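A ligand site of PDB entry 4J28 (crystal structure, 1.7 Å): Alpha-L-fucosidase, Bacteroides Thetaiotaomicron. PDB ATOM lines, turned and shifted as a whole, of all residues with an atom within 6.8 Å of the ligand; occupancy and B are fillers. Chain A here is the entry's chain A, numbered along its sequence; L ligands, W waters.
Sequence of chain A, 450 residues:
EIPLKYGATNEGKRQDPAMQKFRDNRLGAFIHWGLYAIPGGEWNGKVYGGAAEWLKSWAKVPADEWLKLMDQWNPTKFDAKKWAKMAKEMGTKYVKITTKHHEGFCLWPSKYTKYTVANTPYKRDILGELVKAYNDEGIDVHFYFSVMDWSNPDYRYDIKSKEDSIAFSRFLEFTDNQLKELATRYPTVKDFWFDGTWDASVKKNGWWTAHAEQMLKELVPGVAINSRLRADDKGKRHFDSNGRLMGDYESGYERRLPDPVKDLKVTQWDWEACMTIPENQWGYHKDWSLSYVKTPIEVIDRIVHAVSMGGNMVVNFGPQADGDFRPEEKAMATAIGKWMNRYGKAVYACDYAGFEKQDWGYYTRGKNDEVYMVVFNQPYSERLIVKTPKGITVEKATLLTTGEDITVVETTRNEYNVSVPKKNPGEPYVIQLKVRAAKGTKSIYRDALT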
ATOM      1  N   PHE A  30      -5.023  -6.669 -17.964  1.00  0.00           N
ATOM      2  CA  PHE A  30      -3.914  -7.429 -17.455  1.00  0.00           C
ATOM      3  C   PHE A  30      -2.841  -7.417 -18.552  1.00  0.00           C
ATOM      4  O   PHE A  30      -3.196  -7.466 -19.718  1.00  0.00           O
ATOM      5  CB  PHE A  30      -4.342  -8.875 -17.211  1.00  0.00           C
ATOM      6  CG  PHE A  30      -3.833  -9.437 -15.947  1.00  0.00           C
ATOM      7  CD1 PHE A  30      -2.479  -9.494 -15.714  1.00  0.00           C
ATOM      8  CD2 PHE A  30      -4.694  -9.951 -15.009  1.00  0.00           C
ATOM      9  CE1 PHE A  30      -1.988 -10.007 -14.518  1.00  0.00           C
ATOM     10  CE2 PHE A  30      -4.204 -10.453 -13.782  1.00  0.00           C
ATOM     11  CZ  PHE A  30      -2.837 -10.467 -13.564  1.00  0.00           C
ATOM     12  N   HIS A  32       0.502  -9.618 -19.541  1.00  0.00           N
ATOM     13  CA  HIS A  32       1.475 -10.761 -19.373  1.00  0.00           C
ATOM     14  C   HIS A  32       2.560 -10.578 -20.383  1.00  0.00           C
ATOM     15  O   HIS A  32       2.322 -10.672 -21.591  1.00  0.00           O
ATOM     16  CB  HIS A  32       0.822 -12.116 -19.592  1.00  0.00           C
ATOM     17  CG  HIS A  32       0.166 -12.672 -18.381  1.00  0.00           C
ATOM     18  ND1 HIS A  32      -1.017 -12.170 -17.860  1.00  0.00           N
ATOM     19  CD2 HIS A  32       0.528 -13.703 -17.577  1.00  0.00           C
ATOM     20  CE1 HIS A  32      -1.310 -12.831 -16.747  1.00  0.00           C
ATOM     21  NE2 HIS A  32      -0.378 -13.742 -16.544  1.00  0.00           N
ATOM     22  N   ALA A  51      -0.407 -23.081 -22.704  1.00  0.00           N
ATOM     23  CA  ALA A  51      -0.277 -21.646 -22.467  1.00  0.00           C
ATOM     24  C   ALA A  51       1.152 -21.217 -22.751  1.00  0.00           C
ATOM     25  O   ALA A  51       2.100 -21.840 -22.269  1.00  0.00           O
ATOM     26  CB  ALA A  51      -0.687 -21.306 -21.032  1.00  0.00           C
ATOM     27  N   GLU A  53       3.112 -18.864 -21.882  1.00  0.00           N
ATOM     28  CA  GLU A  53       3.952 -18.449 -20.781  1.00  0.00           C
ATOM     29  C   GLU A  53       4.513 -19.628 -19.986  1.00  0.00           C
ATOM     30  O   GLU A  53       5.390 -19.433 -19.161  1.00  0.00           O
ATOM     31  CB  GLU A  53       3.258 -17.420 -19.866  1.00  0.00           C
ATOM     32  CG  GLU A  53       2.137 -17.950 -18.999  1.00  0.00           C
ATOM     33  CD  GLU A  53       0.807 -18.212 -19.711  1.00  0.00           C
ATOM     34  OE1 GLU A  53       0.624 -17.910 -20.919  1.00  0.00           O
ATOM     35  OE2 GLU A  53      -0.063 -18.728 -18.996  1.00  0.00           O
ATOM     36  N   TRP A  54       3.975 -20.831 -20.250  1.00  0.00           N
ATOM     37  CA  TRP A  54       4.445 -22.109 -19.697  1.00  0.00           C
ATOM     38  C   TRP A  54       5.299 -22.934 -20.677  1.00  0.00           C
ATOM     39  O   TRP A  54       5.559 -24.114 -20.423  1.00  0.00           O
ATOM     40  CB  TRP A  54       3.233 -22.970 -19.283  1.00  0.00           C
ATOM     41  CG  TRP A  54       2.715 -22.648 -17.912  1.00  0.00           C
ATOM     42  CD1 TRP A  54       1.955 -21.558 -17.535  1.00  0.00           C
ATOM     43  CD2 TRP A  54       2.906 -23.437 -16.754  1.00  0.00           C
ATOM     44  NE1 TRP A  54       1.691 -21.632 -16.177  1.00  0.00           N
ATOM     45  CE2 TRP A  54       2.278 -22.756 -15.678  1.00  0.00           C
ATOM     46  CE3 TRP A  54       3.592 -24.638 -16.492  1.00  0.00           C
ATOM     47  CZ2 TRP A  54       2.320 -23.240 -14.381  1.00  0.00           C
ATOM     48  CZ3 TRP A  54       3.599 -25.120 -15.208  1.00  0.00           C
ATOM     49  CH2 TRP A  54       2.962 -24.432 -14.174  1.00  0.00           C
ATOM     50  N   THR A  98       2.465  -8.144 -14.988  1.00  0.00           N
ATOM     51  CA  THR A  98       3.403  -9.241 -14.568  1.00  0.00           C
ATOM     52  C   THR A  98       4.780  -8.628 -14.286  1.00  0.00           C
ATOM     53  O   THR A  98       5.522  -8.316 -15.194  1.00  0.00           O
ATOM     54  CB  THR A  98       3.602 -10.346 -15.637  1.00  0.00           C
ATOM     55  OG1 THR A  98       3.976  -9.762 -16.888  1.00  0.00           O
ATOM     56  CG2 THR A  98       2.390 -11.211 -15.850  1.00  0.00           C
ATOM     57  N   HIS A 101       6.961 -13.431 -13.780  1.00  0.00           N
ATOM     58  CA  HIS A 101       6.157 -14.656 -13.925  1.00  0.00           C
ATOM     59  C   HIS A 101       6.974 -15.875 -13.397  1.00  0.00           C
ATOM     60  O   HIS A 101       8.023 -15.702 -12.736  1.00  0.00           O
ATOM     61  CB  HIS A 101       5.646 -14.819 -15.371  1.00  0.00           C
ATOM     62  CG  HIS A 101       4.343 -15.588 -15.455  1.00  0.00           C
ATOM     63  ND1 HIS A 101       4.316 -16.948 -15.734  1.00  0.00           N
ATOM     64  CD2 HIS A 101       3.047 -15.209 -15.301  1.00  0.00           C
ATOM     65  CE1 HIS A 101       3.065 -17.370 -15.692  1.00  0.00           C
ATOM     66  NE2 HIS A 101       2.267 -16.337 -15.445  1.00  0.00           N
ATOM     67  N   HIS A 102       6.464 -17.096 -13.619  1.00  0.00           N
ATOM     68  CA  HIS A 102       7.100 -18.297 -13.060  1.00  0.00           C
ATOM     69  C   HIS A 102       8.537 -18.411 -13.540  1.00  0.00           C
ATOM     70  O   HIS A 102       9.416 -18.799 -12.794  1.00  0.00           O
ATOM     71  CB  HIS A 102       6.338 -19.600 -13.388  1.00  0.00           C
ATOM     72  CG  HIS A 102       4.864 -19.564 -13.112  1.00  0.00           C
ATOM     73  ND1 HIS A 102       4.307 -18.923 -12.031  1.00  0.00           N
ATOM     74  CD2 HIS A 102       3.834 -20.183 -13.747  1.00  0.00           C
ATOM     75  CE1 HIS A 102       2.993 -19.090 -12.046  1.00  0.00           C
ATOM     76  NE2 HIS A 102       2.685 -19.885 -13.047  1.00  0.00           N
ATOM     77  N   TYR A 144       1.216  -8.015 -10.516  1.00  0.00           N
ATOM     78  CA  TYR A 144       1.193  -9.470 -10.469  1.00  0.00           C
ATOM     79  C   TYR A 144       2.592  -9.912 -10.020  1.00  0.00           C
ATOM     80  O   TYR A 144       3.608  -9.392 -10.496  1.00  0.00           O
ATOM     81  CB  TYR A 144       0.905 -10.025 -11.892  1.00  0.00           C
ATOM     82  CG  TYR A 144       1.173 -11.510 -12.066  1.00  0.00           C
ATOM     83  CD1 TYR A 144       2.482 -12.025 -12.018  1.00  0.00           C
ATOM     84  CD2 TYR A 144       0.139 -12.395 -12.280  1.00  0.00           C
ATOM     85  CE1 TYR A 144       2.714 -13.368 -12.205  1.00  0.00           C
ATOM     86  CE2 TYR A 144       0.383 -13.766 -12.437  1.00  0.00           C
ATOM     87  CZ  TYR A 144       1.661 -14.242 -12.350  1.00  0.00           C
ATOM     88  OH  TYR A 144       1.927 -15.577 -12.481  1.00  0.00           O
ATOM     89  N   MET A 148       6.306 -18.851  -6.844  1.00  0.00           N
ATOM     90  CA  MET A 148       7.040 -19.869  -7.612  1.00  0.00           C
ATOM     91  C   MET A 148       7.975 -19.205  -8.620  1.00  0.00           C
ATOM     92  O   MET A 148       7.555 -18.338  -9.404  1.00  0.00           O
ATOM     93  CB  MET A 148       6.092 -20.836  -8.328  1.00  0.00           C
ATOM     94  CG  MET A 148       6.777 -21.894  -9.156  1.00  0.00           C
ATOM     95  SD  MET A 148       5.629 -23.231  -9.663  1.00  0.00           S
ATOM     96  CE  MET A 148       4.667 -22.360 -10.894  1.00  0.00           C
ATOM     97  N   TRP A 193      -1.021  -8.867  -6.603  1.00  0.00           N
ATOM     98  CA  TRP A 193      -1.813 -10.011  -7.043  1.00  0.00           C
ATOM     99  C   TRP A 193      -0.829 -11.190  -7.170  1.00  0.00           C
ATOM    100  O   TRP A 193      -0.052 -11.302  -8.089  1.00  0.00           O
ATOM    101  CB  TRP A 193      -2.524  -9.666  -8.360  1.00  0.00           C
ATOM    102  CG  TRP A 193      -3.633 -10.617  -8.739  1.00  0.00           C
ATOM    103  CD1 TRP A 193      -4.984 -10.436  -8.517  1.00  0.00           C
ATOM    104  CD2 TRP A 193      -3.510 -11.868  -9.456  1.00  0.00           C
ATOM    105  NE1 TRP A 193      -5.688 -11.514  -9.022  1.00  0.00           N
ATOM    106  CE2 TRP A 193      -4.828 -12.399  -9.613  1.00  0.00           C
ATOM    107  CE3 TRP A 193      -2.422 -12.603  -9.978  1.00  0.00           C
ATOM    108  CZ2 TRP A 193      -5.085 -13.624 -10.270  1.00  0.00           C
ATOM    109  CZ3 TRP A 193      -2.688 -13.834 -10.637  1.00  0.00           C
ATOM    110  CH2 TRP A 193      -4.005 -14.318 -10.749  1.00  0.00           C
ATOM    111  N   ASP A 195       0.557 -15.050  -7.454  1.00  0.00           N
ATOM    112  CA  ASP A 195       0.350 -16.291  -8.147  1.00  0.00           C
ATOM    113  C   ASP A 195       1.416 -17.286  -7.734  1.00  0.00           C
ATOM    114  O   ASP A 195       2.418 -16.918  -7.142  1.00  0.00           O
ATOM    115  CB  ASP A 195       0.406 -16.025  -9.664  1.00  0.00           C
ATOM    116  CG  ASP A 195      -0.381 -17.032 -10.496  1.00  0.00           C
ATOM    117  OD1 ASP A 195      -1.162 -17.832  -9.916  1.00  0.00           O
ATOM    118  OD2 ASP A 195      -0.192 -17.006 -11.725  1.00  0.00           O
ATOM    119  N   GLY A 196       1.225 -18.568  -8.085  1.00  0.00           N
ATOM    120  CA  GLY A 196       2.256 -19.572  -7.848  1.00  0.00           C
ATOM    121  C   GLY A 196       2.535 -19.796  -6.370  1.00  0.00           C
ATOM    122  O   GLY A 196       3.690 -19.871  -5.939  1.00  0.00           O
ATOM    123  N   TRP A 198       0.559 -22.262  -4.744  1.00  0.00           N
ATOM    124  CA  TRP A 198      -0.229 -23.518  -4.517  1.00  0.00           C
ATOM    125  C   TRP A 198       0.627 -24.724  -4.054  1.00  0.00           C
ATOM    126  O   TRP A 198       0.078 -25.743  -3.647  1.00  0.00           O
ATOM    127  CB  TRP A 198      -1.029 -23.918  -5.774  1.00  0.00           C
ATOM    128  CG  TRP A 198      -0.151 -24.012  -6.943  1.00  0.00           C
ATOM    129  CD1 TRP A 198       0.795 -24.967  -7.156  1.00  0.00           C
ATOM    130  CD2 TRP A 198      -0.044 -23.078  -8.014  1.00  0.00           C
ATOM    131  NE1 TRP A 198       1.451 -24.716  -8.322  1.00  0.00           N
ATOM    132  CE2 TRP A 198       0.974 -23.547  -8.865  1.00  0.00           C
ATOM    133  CE3 TRP A 198      -0.721 -21.893  -8.337  1.00  0.00           C
ATOM    134  CZ2 TRP A 198       1.337 -22.889 -10.041  1.00  0.00           C
ATOM    135  CZ3 TRP A 198      -0.377 -21.235  -9.535  1.00  0.00           C
ATOM    136  CH2 TRP A 198       0.646 -21.725 -10.346  1.00  0.00           C
ATOM    137  N   ARG A 228      -5.348 -15.247  -3.275  1.00  0.00           N
ATOM    138  CA  ARG A 228      -4.515 -16.338  -3.734  1.00  0.00           C
ATOM    139  C   ARG A 228      -3.184 -16.439  -2.993  1.00  0.00           C
ATOM    140  O   ARG A 228      -2.540 -17.511  -2.948  1.00  0.00           O
ATOM    141  CB  ARG A 228      -4.274 -16.183  -5.249  1.00  0.00           C
ATOM    142  CG  ARG A 228      -3.495 -17.316  -5.870  1.00  0.00           C
ATOM    143  CD  ARG A 228      -3.645 -17.317  -7.382  1.00  0.00           C
ATOM    144  NE  ARG A 228      -4.927 -17.893  -7.801  1.00  0.00           N
ATOM    145  CZ  ARG A 228      -5.882 -17.306  -8.529  1.00  0.00           C
ATOM    146  NH1 ARG A 228      -5.726 -16.081  -8.964  1.00  0.00           N
ATOM    147  NH2 ARG A 228      -6.994 -17.979  -8.836  1.00  0.00           N
ATOM    148  N   GLU A 254     -11.452 -17.381 -13.191  1.00  0.00           N
ATOM    149  CA  GLU A 254     -10.663 -17.177 -14.416  1.00  0.00           C
ATOM    150  C   GLU A 254     -11.348 -17.753 -15.654  1.00  0.00           C
ATOM    151  O   GLU A 254     -11.496 -17.092 -16.677  1.00  0.00           O
ATOM    152  CB  GLU A 254      -9.278 -17.799 -14.297  1.00  0.00           C
ATOM    153  CG  GLU A 254      -8.313 -17.225 -13.239  1.00  0.00           C
ATOM    154  CD  GLU A 254      -6.883 -17.840 -13.347  1.00  0.00           C
ATOM    155  OE1 GLU A 254      -6.649 -18.657 -14.257  1.00  0.00           O
ATOM    156  OE2 GLU A 254      -5.959 -17.534 -12.558  1.00  0.00           O
ATOM    157  N   CYS A 274     -10.313 -12.454 -13.646  1.00  0.00           N
ATOM    158  CA  CYS A 274      -9.375 -12.150 -14.714  1.00  0.00           C
ATOM    159  C   CYS A 274      -9.643 -13.117 -15.897  1.00  0.00           C
ATOM    160  O   CYS A 274      -9.936 -14.270 -15.684  1.00  0.00           O
ATOM    161  CB  CYS A 274      -7.936 -12.194 -14.188  1.00  0.00           C
ATOM    162  SG  CYS A 274      -7.504 -11.118 -12.755  1.00  0.00           S
ATOM    163  N   ASN A 280      -7.098 -20.144 -23.383  1.00  0.00           N
ATOM    164  CA  ASN A 280      -6.130 -20.318 -22.316  1.00  0.00           C
ATOM    165  C   ASN A 280      -4.715 -19.930 -22.787  1.00  0.00           C
ATOM    166  O   ASN A 280      -3.832 -20.761 -22.865  1.00  0.00           O
ATOM    167  CB  ASN A 280      -6.107 -21.752 -21.767  1.00  0.00           C
ATOM    168  CG  ASN A 280      -5.272 -21.880 -20.499  1.00  0.00           C
ATOM    169  OD1 ASN A 280      -4.964 -20.906 -19.796  1.00  0.00           O
ATOM    170  ND2 ASN A 280      -4.831 -23.091 -20.226  1.00  0.00           N
ATOM    171  N   TRP A 282      -2.176 -16.616 -21.872  1.00  0.00           N
ATOM    172  CA  TRP A 282      -1.951 -15.364 -21.185  1.00  0.00           C
ATOM    173  C   TRP A 282      -0.800 -14.596 -21.816  1.00  0.00           C
ATOM    174  O   TRP A 282      -0.973 -13.431 -22.254  1.00  0.00           O
ATOM    175  CB  TRP A 282      -1.742 -15.596 -19.685  1.00  0.00           C
ATOM    176  CG  TRP A 282      -2.845 -16.231 -18.977  1.00  0.00           C
ATOM    177  CD1 TRP A 282      -3.070 -17.576 -18.823  1.00  0.00           C
ATOM    178  CD2 TRP A 282      -3.884 -15.562 -18.223  1.00  0.00           C
ATOM    179  NE1 TRP A 282      -4.146 -17.773 -18.035  1.00  0.00           N
ATOM    180  CE2 TRP A 282      -4.691 -16.564 -17.673  1.00  0.00           C
ATOM    181  CE3 TRP A 282      -4.204 -14.227 -17.977  1.00  0.00           C
ATOM    182  CZ2 TRP A 282      -5.796 -16.277 -16.838  1.00  0.00           C
ATOM    183  CZ3 TRP A 282      -5.346 -13.937 -17.216  1.00  0.00           C
ATOM    184  CH2 TRP A 282      -6.125 -14.946 -16.663  1.00  0.00           C
ATOM    185  N   GLY A 283       0.398 -15.212 -21.870  1.00  0.00           N
ATOM    186  CA  GLY A 283       1.488 -14.643 -22.687  1.00  0.00           C
ATOM    187  C   GLY A 283       1.180 -14.706 -24.152  1.00  0.00           C
ATOM    188  O   GLY A 283       0.263 -15.411 -24.590  1.00  0.00           O
HETATM  189  O1  LIG L   1       0.221 -18.554 -16.433  1.00  0.00           O
HETATM  190  C1  LIG L   1      -1.043 -18.314 -15.751  1.00  0.00           C
HETATM  191  C2  LIG L   1      -1.479 -16.848 -15.638  1.00  0.00           C
HETATM  192  O2  LIG L   1      -0.470 -16.054 -15.081  1.00  0.00           O
HETATM  193  C3  LIG L   1      -2.679 -16.994 -14.709  1.00  0.00           C
HETATM  194  C4  LIG L   1      -3.211 -15.626 -14.302  1.00  0.00           C
HETATM  195  N1  LIG L   1      -2.130 -17.857 -13.657  1.00  0.00           N
HETATM  196  C5  LIG L   1      -0.961 -18.670 -14.307  1.00  0.00           C
HETATM  197  C6  LIG L   1      -1.161 -20.189 -14.033  1.00  0.00           C
HETATM  198  N2  LIG L   1      -0.340 -21.021 -13.371  1.00  0.00           N
HETATM  199  C7  LIG L   1      -0.974 -22.216 -13.302  1.00  0.00           C
HETATM  200  C8  LIG L   1      -0.628 -23.417 -12.777  1.00  0.00           C
HETATM  201  C9  LIG L   1      -1.489 -24.526 -12.858  1.00  0.00           C
HETATM  202  C10 LIG L   1      -2.721 -24.366 -13.493  1.00  0.00           C
HETATM  203  C11 LIG L   1      -3.016 -23.110 -14.028  1.00  0.00           C
HETATM  204  C12 LIG L   1      -2.149 -22.092 -13.933  1.00  0.00           C
HETATM  205  N3  LIG L   1      -2.249 -20.835 -14.365  1.00  0.00           N
HETATM  206  O   HOH W   1      -1.747 -20.950 -17.953  1.00  0.00           O
HETATM  207  O   HOH W   2      -3.551 -19.123 -10.796  1.00  0.00           O
HETATM  208  O   HOH W   3      -4.904 -20.080 -15.790  1.00  0.00           O
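A nitrogen (N1) of the ligand lies within salt-bridge range of the side-chain carboxylate of Asp 195 (2.9 Å). NE2 of His 32 sits at hydrogen-bond distance from O2 of the ligand. N2 of the ligand sits at hydrogen-bond distance from NE2 of His 102 (3.2 Å). OE2 of Glu 53 lies within hydrogen-bond range of O1 of the ligand, 2.6 Å away. The indole nitrogen of Trp 54 sits at hydrogen-bond distance from an oxygen (O1) of the ligand, at 3.4 Å. A ring nitrogen (NE2) of His 101 sits at hydrogen-bond distance from an oxygen (O2) of the ligand (2.8 Å). The side-chain carboxylate (OE2) of Glu 254 lies within salt-bridge range of a nitrogen (N1) of the ligand (3.997 Å).
The side-chain carboxylate of Glu 53 lies within hydrogen-bond range of the backbone NH of Gly 283 (2.9 Å). The side-chain carboxylate of Glu 254 lies within salt-bridge range of the guanidinium group of Arg 228, at 3.9 Å. The side-chain hydroxyl of Tyr 144 sits at hydrogen-bond distance from the side-chain carboxylate of Asp 195 (2.7 Å). A ring nitrogen (NE2) of His 101 sits close to the side-chain hydroxyl (OH) of Tyr 144 (3.1 Å). OE1 of Glu 53 lies within hydrogen-bond range of N of Trp 282 (3.2 Å).
OH of Tyr 144 touches O2 of the ligand, at 3.6 Å. Trp 193 touches the ligand. Trp 198 touches the ligand. Trp 282 touches the ligand. Hydrophobic or aromatic side chains within 4 Å of the ligand: His 32, Trp 54, His 101, Tyr 144, Trp 193, Trp 198 and Trp 282.
Water W3 lies within hydrogen-bond range of OE1 of Glu 254, N3 of the ligand and NE1 of Trp 282. Water W2 lies within hydrogen-bond range of the side-chain carboxylate (OD1) of Asp 195 (2.9 Å), the side-chain carboxylate (OE2) of Glu 254 (3.4 Å) and a nitrogen (N1) of the ligand (3.4 Å). Water W1 lies within hydrogen-bond range of the side-chain carboxylate of Glu 53 (3.0 Å) and an oxygen (O1) of the ligand (3.5 Å).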
